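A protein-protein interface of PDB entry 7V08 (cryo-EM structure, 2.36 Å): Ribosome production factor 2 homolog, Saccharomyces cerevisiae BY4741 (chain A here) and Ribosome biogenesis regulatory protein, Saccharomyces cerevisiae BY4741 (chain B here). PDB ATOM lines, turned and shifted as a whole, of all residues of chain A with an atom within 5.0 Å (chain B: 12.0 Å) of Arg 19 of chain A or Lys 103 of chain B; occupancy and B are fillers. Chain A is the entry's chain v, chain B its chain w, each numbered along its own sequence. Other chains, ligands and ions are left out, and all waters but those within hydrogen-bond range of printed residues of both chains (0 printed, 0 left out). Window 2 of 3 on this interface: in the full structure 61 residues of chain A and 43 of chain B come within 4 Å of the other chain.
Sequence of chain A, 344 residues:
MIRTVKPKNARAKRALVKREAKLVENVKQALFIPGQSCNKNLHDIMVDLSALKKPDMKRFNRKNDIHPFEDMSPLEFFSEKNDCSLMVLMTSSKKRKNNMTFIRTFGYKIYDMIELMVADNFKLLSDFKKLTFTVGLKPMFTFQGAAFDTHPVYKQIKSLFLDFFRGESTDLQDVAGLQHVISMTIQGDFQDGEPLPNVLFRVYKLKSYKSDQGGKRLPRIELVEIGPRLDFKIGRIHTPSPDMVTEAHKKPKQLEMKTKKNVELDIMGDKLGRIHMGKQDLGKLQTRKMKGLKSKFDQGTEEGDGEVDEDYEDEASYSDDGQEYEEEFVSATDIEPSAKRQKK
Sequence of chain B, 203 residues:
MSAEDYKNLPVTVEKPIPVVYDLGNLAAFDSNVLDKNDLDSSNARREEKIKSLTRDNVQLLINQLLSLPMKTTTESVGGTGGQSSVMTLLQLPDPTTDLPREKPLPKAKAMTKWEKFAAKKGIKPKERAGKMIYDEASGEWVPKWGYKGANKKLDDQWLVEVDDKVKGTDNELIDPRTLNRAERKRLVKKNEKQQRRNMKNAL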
ATOM      1  N   ALA A  15      29.301  35.066 -22.667  1.00  0.00           N
ATOM      2  CA  ALA A  15      29.836  33.899 -21.969  1.00  0.00           C
ATOM      3  C   ALA A  15      28.991  33.542 -20.749  1.00  0.00           C
ATOM      4  O   ALA A  15      28.772  32.361 -20.459  1.00  0.00           O
ATOM      5  CB  ALA A  15      31.288  34.154 -21.564  1.00  0.00           C
ATOM      6  N   LEU A  16      28.501  34.551 -20.027  1.00  0.00           N
ATOM      7  CA  LEU A  16      27.629  34.284 -18.885  1.00  0.00           C
ATOM      8  C   LEU A  16      26.328  33.614 -19.316  1.00  0.00           C
ATOM      9  O   LEU A  16      25.858  32.675 -18.661  1.00  0.00           O
ATOM     10  CB  LEU A  16      27.331  35.582 -18.134  1.00  0.00           C
ATOM     11  CG  LEU A  16      28.497  36.239 -17.398  1.00  0.00           C
ATOM     12  CD1 LEU A  16      28.048  37.533 -16.750  1.00  0.00           C
ATOM     13  CD2 LEU A  16      29.079  35.288 -16.360  1.00  0.00           C
ATOM     14  N   VAL A  17      25.728  34.089 -20.408  1.00  0.00           N
ATOM     15  CA  VAL A  17      24.483  33.490 -20.886  1.00  0.00           C
ATOM     16  C   VAL A  17      24.733  32.074 -21.395  1.00  0.00           C
ATOM     17  O   VAL A  17      23.886  31.186 -21.242  1.00  0.00           O
ATOM     18  CB  VAL A  17      23.830  34.381 -21.956  1.00  0.00           C
ATOM     19  CG1 VAL A  17      22.554  33.749 -22.478  1.00  0.00           C
ATOM     20  CG2 VAL A  17      23.520  35.744 -21.383  1.00  0.00           C
ATOM     21  N   LYS A  18      25.895  31.841 -22.009  1.00  0.00           N
ATOM     22  CA  LYS A  18      26.261  30.481 -22.390  1.00  0.00           C
ATOM     23  C   LYS A  18      26.385  29.586 -21.165  1.00  0.00           C
ATOM     24  O   LYS A  18      26.000  28.413 -21.203  1.00  0.00           O
ATOM     25  CB  LYS A  18      27.569  30.490 -23.177  1.00  0.00           C
ATOM     26  CG  LYS A  18      27.764  29.270 -24.045  1.00  0.00           C
ATOM     27  CD  LYS A  18      29.130  29.276 -24.704  1.00  0.00           C
ATOM     28  CE  LYS A  18      29.359  30.548 -25.506  1.00  0.00           C
ATOM     29  NZ  LYS A  18      30.684  30.530 -26.191  1.00  0.00           N
ATOM     30  N   ARG A  19      26.915  30.128 -20.067  1.00  0.00           N
ATOM     31  CA  ARG A  19      27.083  29.347 -18.846  1.00  0.00           C
ATOM     32  C   ARG A  19      25.757  29.058 -18.149  1.00  0.00           C
ATOM     33  O   ARG A  19      25.613  27.999 -17.528  1.00  0.00           O
ATOM     34  CB  ARG A  19      28.036  30.081 -17.896  1.00  0.00           C
ATOM     35  CG  ARG A  19      28.505  29.264 -16.706  1.00  0.00           C
ATOM     36  CD  ARG A  19      29.923  29.643 -16.283  1.00  0.00           C
ATOM     37  NE  ARG A  19      30.868  29.496 -17.383  1.00  0.00           N
ATOM     38  CZ  ARG A  19      32.186  29.438 -17.244  1.00  0.00           C
ATOM     39  NH1 ARG A  19      32.761  29.499 -16.054  1.00  0.00           N
ATOM     40  NH2 ARG A  19      32.945  29.304 -18.327  1.00  0.00           N
ATOM     41  N   GLU A  20      24.782  29.959 -18.254  1.00  0.00           N
ATOM     42  CA  GLU A  20      23.544  29.828 -17.490  1.00  0.00           C
ATOM     43  C   GLU A  20      22.704  28.641 -17.977  1.00  0.00           C
ATOM     44  O   GLU A  20      22.956  28.047 -19.028  1.00  0.00           O
ATOM     45  CB  GLU A  20      22.722  31.114 -17.563  1.00  0.00           C
ATOM     46  CG  GLU A  20      21.811  31.221 -18.786  1.00  0.00           C
ATOM     47  CD  GLU A  20      21.129  32.569 -18.884  1.00  0.00           C
ATOM     48  OE1 GLU A  20      21.390  33.435 -18.025  1.00  0.00           O
ATOM     49  OE2 GLU A  20      20.331  32.770 -19.823  1.00  0.00           O
ATOM     50  N   ALA A  21      21.696  28.295 -17.176  1.00  0.00           N
ATOM     51  CA  ALA A  21      20.833  27.156 -17.458  1.00  0.00           C
ATOM     52  C   ALA A  21      19.880  27.450 -18.615  1.00  0.00           C
ATOM     53  O   ALA A  21      19.566  28.603 -18.924  1.00  0.00           O
ATOM     54  CB  ALA A  21      20.032  26.772 -16.214  1.00  0.00           C
ATOM     55  N   GLU A  25      19.561  21.704 -23.305  1.00  0.00           N
ATOM     56  CA  GLU A  25      20.939  21.902 -22.889  1.00  0.00           C
ATOM     57  C   GLU A  25      21.915  21.746 -24.049  1.00  0.00           C
ATOM     58  O   GLU A  25      21.602  21.185 -25.102  1.00  0.00           O
ATOM     59  CB  GLU A  25      21.311  20.925 -21.773  1.00  0.00           C
ATOM     60  CG  GLU A  25      20.896  21.405 -20.398  1.00  0.00           C
ATOM     61  CD  GLU A  25      21.419  22.802 -20.098  1.00  0.00           C
ATOM     62  OE1 GLU A  25      22.596  23.087 -20.419  1.00  0.00           O
ATOM     63  OE2 GLU A  25      20.648  23.614 -19.548  1.00  0.00           O
ATOM     64  N   GLU A  80      32.884  24.418 -11.792  1.00  0.00           N
ATOM     65  CA  GLU A  80      32.224  25.713 -11.911  1.00  0.00           C
ATOM     66  C   GLU A  80      33.063  26.696 -12.715  1.00  0.00           C
ATOM     67  O   GLU A  80      32.508  27.554 -13.411  1.00  0.00           O
ATOM     68  CB  GLU A  80      31.905  26.274 -10.523  1.00  0.00           C
ATOM     69  CG  GLU A  80      31.173  27.612 -10.546  1.00  0.00           C
ATOM     70  CD  GLU A  80      30.540  27.968  -9.217  1.00  0.00           C
ATOM     71  OE1 GLU A  80      30.788  27.254  -8.224  1.00  0.00           O
ATOM     72  OE2 GLU A  80      29.784  28.961  -9.163  1.00  0.00           O
ATOM     73  N   LYS A  81      34.393  26.583 -12.654  1.00  0.00           N
ATOM     74  CA  LYS A  81      35.228  27.487 -13.434  1.00  0.00           C
ATOM     75  C   LYS A  81      35.192  27.150 -14.918  1.00  0.00           C
ATOM     76  O   LYS A  81      35.103  28.050 -15.761  1.00  0.00           O
ATOM     77  CB  LYS A  81      36.665  27.457 -12.920  1.00  0.00           C
ATOM     78  CG  LYS A  81      36.861  28.201 -11.621  1.00  0.00           C
ATOM     79  CD  LYS A  81      36.206  29.563 -11.674  1.00  0.00           C
ATOM     80  CE  LYS A  81      36.885  30.526 -10.734  1.00  0.00           C
ATOM     81  NZ  LYS A  81      36.204  31.851 -10.723  1.00  0.00           N
ATOM     82  N   ASN A  82      35.262  25.868 -15.261  1.00  0.00           N
ATOM     83  CA  ASN A  82      35.422  25.443 -16.641  1.00  0.00           C
ATOM     84  C   ASN A  82      34.104  25.181 -17.352  1.00  0.00           C
ATOM     85  O   ASN A  82      34.121  24.909 -18.558  1.00  0.00           O
ATOM     86  CB  ASN A  82      36.290  24.181 -16.702  1.00  0.00           C
ATOM     87  CG  ASN A  82      37.672  24.388 -16.114  1.00  0.00           C
ATOM     88  OD1 ASN A  82      38.647  24.562 -16.840  1.00  0.00           O
ATOM     89  ND2 ASN A  82      37.764  24.363 -14.791  1.00  0.00           N
ATOM     90  N   ASP A  83      32.971  25.253 -16.641  1.00  0.00           N
ATOM     91  CA  ASP A  83      31.655  24.940 -17.206  1.00  0.00           C
ATOM     92  C   ASP A  83      31.645  23.527 -17.782  1.00  0.00           C
ATOM     93  O   ASP A  83      31.061  23.257 -18.832  1.00  0.00           O
ATOM     94  CB  ASP A  83      31.240  25.979 -18.255  1.00  0.00           C
ATOM     95  CG  ASP A  83      29.757  25.941 -18.571  1.00  0.00           C
ATOM     96  OD1 ASP A  83      28.994  25.304 -17.815  1.00  0.00           O
ATOM     97  OD2 ASP A  83      29.356  26.551 -19.583  1.00  0.00           O
ATOM     98  N   PHE A 106      26.097  17.917 -11.148  1.00  0.00           N
ATOM     99  CA  PHE A 106      24.790  18.503 -11.415  1.00  0.00           C
ATOM    100  C   PHE A 106      24.703  19.841 -10.699  1.00  0.00           C
ATOM    101  O   PHE A 106      24.684  19.887  -9.465  1.00  0.00           O
ATOM    102  CB  PHE A 106      23.662  17.576 -10.963  1.00  0.00           C
ATOM    103  CG  PHE A 106      22.318  18.237 -10.928  1.00  0.00           C
ATOM    104  CD1 PHE A 106      21.627  18.492 -12.099  1.00  0.00           C
ATOM    105  CD2 PHE A 106      21.745  18.609  -9.725  1.00  0.00           C
ATOM    106  CE1 PHE A 106      20.392  19.100 -12.071  1.00  0.00           C
ATOM    107  CE2 PHE A 106      20.511  19.222  -9.692  1.00  0.00           C
ATOM    108  CZ  PHE A 106      19.833  19.466 -10.869  1.00  0.00           C
ATOM    109  N   GLY A 107      24.632  20.921 -11.471  1.00  0.00           N
ATOM    110  CA  GLY A 107      24.616  22.258 -10.899  1.00  0.00           C
ATOM    111  C   GLY A 107      25.892  22.633 -10.176  1.00  0.00           C
ATOM    112  O   GLY A 107      25.839  23.305  -9.138  1.00  0.00           O
ATOM    113  N   TYR A 108      27.043  22.219 -10.713  1.00  0.00           N
ATOM    114  CA  TYR A 108      28.376  22.441 -10.142  1.00  0.00           C
ATOM    115  C   TYR A 108      28.561  21.763  -8.786  1.00  0.00           C
ATOM    116  O   TYR A 108      29.515  22.063  -8.065  1.00  0.00           O
ATOM    117  CB  TYR A 108      28.704  23.935 -10.032  1.00  0.00           C
ATOM    118  CG  TYR A 108      28.607  24.668 -11.344  1.00  0.00           C
ATOM    119  CD1 TYR A 108      28.994  24.057 -12.525  1.00  0.00           C
ATOM    120  CD2 TYR A 108      28.120  25.970 -11.404  1.00  0.00           C
ATOM    121  CE1 TYR A 108      28.908  24.714 -13.727  1.00  0.00           C
ATOM    122  CE2 TYR A 108      28.031  26.640 -12.609  1.00  0.00           C
ATOM    123  CZ  TYR A 108      28.427  26.003 -13.766  1.00  0.00           C
ATOM    124  OH  TYR A 108      28.346  26.646 -14.972  1.00  0.00           O
ATOM    125  N   LEU B  99      18.619  10.415 -18.908  1.00  0.00           N
ATOM    126  CA  LEU B  99      19.928  10.744 -18.377  1.00  0.00           C
ATOM    127  C   LEU B  99      19.813  12.008 -17.541  1.00  0.00           C
ATOM    128  O   LEU B  99      18.953  12.853 -17.811  1.00  0.00           O
ATOM    129  CB  LEU B  99      20.943  10.952 -19.512  1.00  0.00           C
ATOM    130  CG  LEU B  99      21.126   9.766 -20.463  1.00  0.00           C
ATOM    131  CD1 LEU B  99      21.760  10.202 -21.769  1.00  0.00           C
ATOM    132  CD2 LEU B  99      21.958   8.681 -19.809  1.00  0.00           C
ATOM    133  N   PRO B 100      20.634  12.150 -16.503  1.00  0.00           N
ATOM    134  CA  PRO B 100      20.560  13.356 -15.673  1.00  0.00           C
ATOM    135  C   PRO B 100      20.977  14.600 -16.440  1.00  0.00           C
ATOM    136  O   PRO B 100      21.833  14.556 -17.325  1.00  0.00           O
ATOM    137  CB  PRO B 100      21.537  13.060 -14.529  1.00  0.00           C
ATOM    138  CG  PRO B 100      22.474  12.052 -15.091  1.00  0.00           C
ATOM    139  CD  PRO B 100      21.657  11.211 -16.015  1.00  0.00           C
ATOM    140  N   ARG B 101      20.350  15.721 -16.094  1.00  0.00           N
ATOM    141  CA  ARG B 101      20.778  17.003 -16.628  1.00  0.00           C
ATOM    142  C   ARG B 101      22.018  17.491 -15.886  1.00  0.00           C
ATOM    143  O   ARG B 101      22.350  17.014 -14.798  1.00  0.00           O
ATOM    144  CB  ARG B 101      19.664  18.047 -16.514  1.00  0.00           C
ATOM    145  CG  ARG B 101      18.361  17.669 -17.190  1.00  0.00           C
ATOM    146  CD  ARG B 101      17.818  18.823 -18.008  1.00  0.00           C
ATOM    147  NE  ARG B 101      17.775  20.070 -17.254  1.00  0.00           N
ATOM    148  CZ  ARG B 101      17.711  21.272 -17.810  1.00  0.00           C
ATOM    149  NH1 ARG B 101      17.679  21.424 -19.123  1.00  0.00           N
ATOM    150  NH2 ARG B 101      17.685  22.347 -17.031  1.00  0.00           N
ATOM    151  N   GLU B 102      22.715  18.451 -16.493  1.00  0.00           N
ATOM    152  CA  GLU B 102      23.885  19.030 -15.847  1.00  0.00           C
ATOM    153  C   GLU B 102      23.536  20.179 -14.910  1.00  0.00           C
ATOM    154  O   GLU B 102      24.334  20.499 -14.024  1.00  0.00           O
ATOM    155  CB  GLU B 102      24.888  19.510 -16.894  1.00  0.00           C
ATOM    156  CG  GLU B 102      24.429  20.699 -17.708  1.00  0.00           C
ATOM    157  CD  GLU B 102      25.263  20.885 -18.952  1.00  0.00           C
ATOM    158  OE1 GLU B 102      26.034  19.960 -19.284  1.00  0.00           O
ATOM    159  OE2 GLU B 102      25.147  21.948 -19.597  1.00  0.00           O
ATOM    160  N   LYS B 103      22.388  20.819 -15.096  1.00  0.00           N
ATOM    161  CA  LYS B 103      21.957  21.931 -14.264  1.00  0.00           C
ATOM    162  C   LYS B 103      20.457  21.828 -14.044  1.00  0.00           C
ATOM    163  O   LYS B 103      19.747  21.243 -14.870  1.00  0.00           O
ATOM    164  CB  LYS B 103      22.300  23.288 -14.904  1.00  0.00           C
ATOM    165  CG  LYS B 103      23.791  23.604 -14.931  1.00  0.00           C
ATOM    166  CD  LYS B 103      24.072  24.996 -15.475  1.00  0.00           C
ATOM    167  CE  LYS B 103      23.766  25.082 -16.958  1.00  0.00           C
ATOM    168  NZ  LYS B 103      24.684  24.262 -17.792  1.00  0.00           N
ATOM    169  N   PRO B 104      19.950  22.363 -12.937  1.00  0.00           N
ATOM    170  CA  PRO B 104      18.500  22.384 -12.732  1.00  0.00           C
ATOM    171  C   PRO B 104      17.812  23.314 -13.719  1.00  0.00           C
ATOM    172  O   PRO B 104      18.430  24.182 -14.335  1.00  0.00           O
ATOM    173  CB  PRO B 104      18.350  22.890 -11.292  1.00  0.00           C
ATOM    174  CG  PRO B 104      19.613  23.599 -11.005  1.00  0.00           C
ATOM    175  CD  PRO B 104      20.670  22.842 -11.746  1.00  0.00           C
ATOM    176  N   LEU B 105      16.507  23.104 -13.867  1.00  0.00           N
ATOM    177  CA  LEU B 105      15.711  23.918 -14.771  1.00  0.00           C
ATOM    178  C   LEU B 105      15.654  25.363 -14.281  1.00  0.00           C
ATOM    179  O   LEU B 105      15.729  25.622 -13.075  1.00  0.00           O
ATOM    180  CB  LEU B 105      14.298  23.357 -14.889  1.00  0.00           C
ATOM    181  CG  LEU B 105      14.138  22.096 -15.733  1.00  0.00           C
ATOM    182  CD1 LEU B 105      12.791  21.457 -15.481  1.00  0.00           C
ATOM    183  CD2 LEU B 105      14.300  22.441 -17.202  1.00  0.00           C
ATOM    184  N   PRO B 106      15.546  26.326 -15.198  1.00  0.00           N
ATOM    185  CA  PRO B 106      15.418  27.728 -14.779  1.00  0.00           C
ATOM    186  C   PRO B 106      14.097  27.959 -14.061  1.00  0.00           C
ATOM    187  O   PRO B 106      13.022  27.815 -14.646  1.00  0.00           O
ATOM    188  CB  PRO B 106      15.482  28.507 -16.099  1.00  0.00           C
ATOM    189  CG  PRO B 106      16.021  27.548 -17.108  1.00  0.00           C
ATOM    190  CD  PRO B 106      15.583  26.194 -16.662  1.00  0.00           C
ATOM    191  N   LYS B 107      14.189  28.304 -12.781  1.00  0.00           N
ATOM    192  CA  LYS B 107      13.009  28.682 -12.023  1.00  0.00           C
ATOM    193  C   LYS B 107      12.495  30.029 -12.508  1.00  0.00           C
ATOM    194  O   LYS B 107      13.259  30.880 -12.974  1.00  0.00           O
ATOM    195  CB  LYS B 107      13.330  28.745 -10.530  1.00  0.00           C
ATOM    196  CG  LYS B 107      13.943  27.470  -9.978  1.00  0.00           C
ATOM    197  CD  LYS B 107      14.136  27.551  -8.473  1.00  0.00           C
ATOM    198  CE  LYS B 107      12.847  27.962  -7.775  1.00  0.00           C
ATOM    199  NZ  LYS B 107      11.710  27.054  -8.080  1.00  0.00           N
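The side-chain carboxylate (OE2) of Glu 25 of chain A is in salt-bridge range of the guanidinium group (NH1) of Arg 101 of chain B (3.7 Å). OE1 of Glu 25 of chain A is in salt-bridge range of NZ of Lys 103 of chain B, at 3.6 Å. The backbone NH (N) of Gly 107 of chain A lies within hydrogen-bond range of the backbone carbonyl oxygen (O) of Glu 102 of chain B, 2.6 Å away. The side-chain carboxylate of Glu 102 of chain B lies close to the side-chain carboxylate of Glu 25 of chain A, at 2.9 Å.
NH1 of Arg 19 of chain A lies within hydrogen-bond range of O of Glu 80 of chain A. NH1 of Arg 19 of chain A lies within hydrogen-bond range of O of Lys 81 of chain A (2.8 Å). The guanidinium group (NE) of Arg 19 of chain A is in salt-bridge range of the side-chain carboxylate (OD2) of Asp 83 of chain A (3.97 Å). The guanidinium group of Arg 101 of chain B is in hydrogen-bond range of the backbone carbonyl oxygen of Lys 103 of chain B, 3.2 Å away. NH2 of Arg 101 of chain B is in hydrogen-bond range of O of Pro 104 of chain B, at 3.3 Å. The side-chain amino group (NZ) of Lys 103 of chain B is in salt-bridge range of the side-chain carboxylate (OE2) of Glu 102 of chain B (3.0 Å).
Arg 19 of chain A touches Lys 103 of chain B (O to CE, 3.5 Å). Glu 20 of chain A touches Lys 103 of chain B. Ala 21 of chain A touches Lys 103 of chain B (CA to CE, 3.6 Å). Pro 104 of chain B touches Ala 21 of chain A (O to CB, 3.6 Å). Arg 101 of chain B touches Phe 106 of chain A (O to CD1, 3.2 Å). Phe 106 of chain A touches Glu 102 of chain B (CA to O, 3.3 Å). Phe 106 of chain A touches Lys 103 of chain B (CE1 to C, 3.4 Å). Phe 106 of chain A touches Pro 104 of chain B. N of Gly 107 of chain A touches CA of Lys 103 of chain B, at 3.997 Å.
Arg 19 of chain A touches just one residue of chain B: Lys 103. Of the printed residues of chain A, Lys 103 of chain B touches Arg 19 (3.5 Å), Glu 20 (3.7 Å), Ala 21 (3.6 Å), Glu 25 (3.6 Å), Phe 106 (3.4 Å) and Gly 107 (3.997 Å). No residue of chain B comes within 4 Å of Lys 18 of chain A. Of chain B, only Lys 103 and Pro 104 come within 4 Å of Ala 21 of chain A. No residue of chain B comes within 4 Å of Asn 82 of chain A. Phe 106 of chain A touches just these residues of chain B: Arg 101, Glu 102, Lys 103 and Pro 104. Of the printed residues of chain B, Glu 25 of chain A touches Arg 101 (3.5 Å), Glu 102 (2.9 Å) and Lys 103 (3.6 Å). Printed residues of chain A within 4 Å of Glu 102 of chain B: Glu 25 (2.9 Å), Phe 106 (3.3 Å) and Gly 107 (2.6 Å). Printed residues of chain A within 4 Å of Pro 104 of chain B: Ala 21 and Phe 106. Of the printed residues of chain A, Arg 101 of chain B touches Glu 25 and Phe 106. Printed residues of chain B within 4 Å of Gly 107 of chain A: Glu 102 and Lys 103. Pro 106 of chain B touches none of the printed residues of chain A. The nearest residue of chain B that does not touch Arg 19 of chain A is Glu 102 of chain B (6.4 Å). The nearest printed residue of chain B that does not touch Gly 107 of chain A is Pro 104 of chain B (4.1 Å).
Hydrophobic or aromatic side chains of chain A within 4 Å of the printed part of chain B: Ala 21 and Phe 106. Of the 9 printed residues of chain B, 4 touch a printed residue of chain A. Hydrophobic or aromatic side chains of chain B within 4 Å of the printed part of chain A: Pro 104. Among the printed residues, 13 pairs touch across the chains. Among the printed residues, Asp or Glu carboxylates within 4 Å of a Lys or Arg side-chain nitrogen of the other chain: Glu 25 of chain A with Arg 101 of chain B and Glu 25 of chain A with Lys 103 of chain B.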
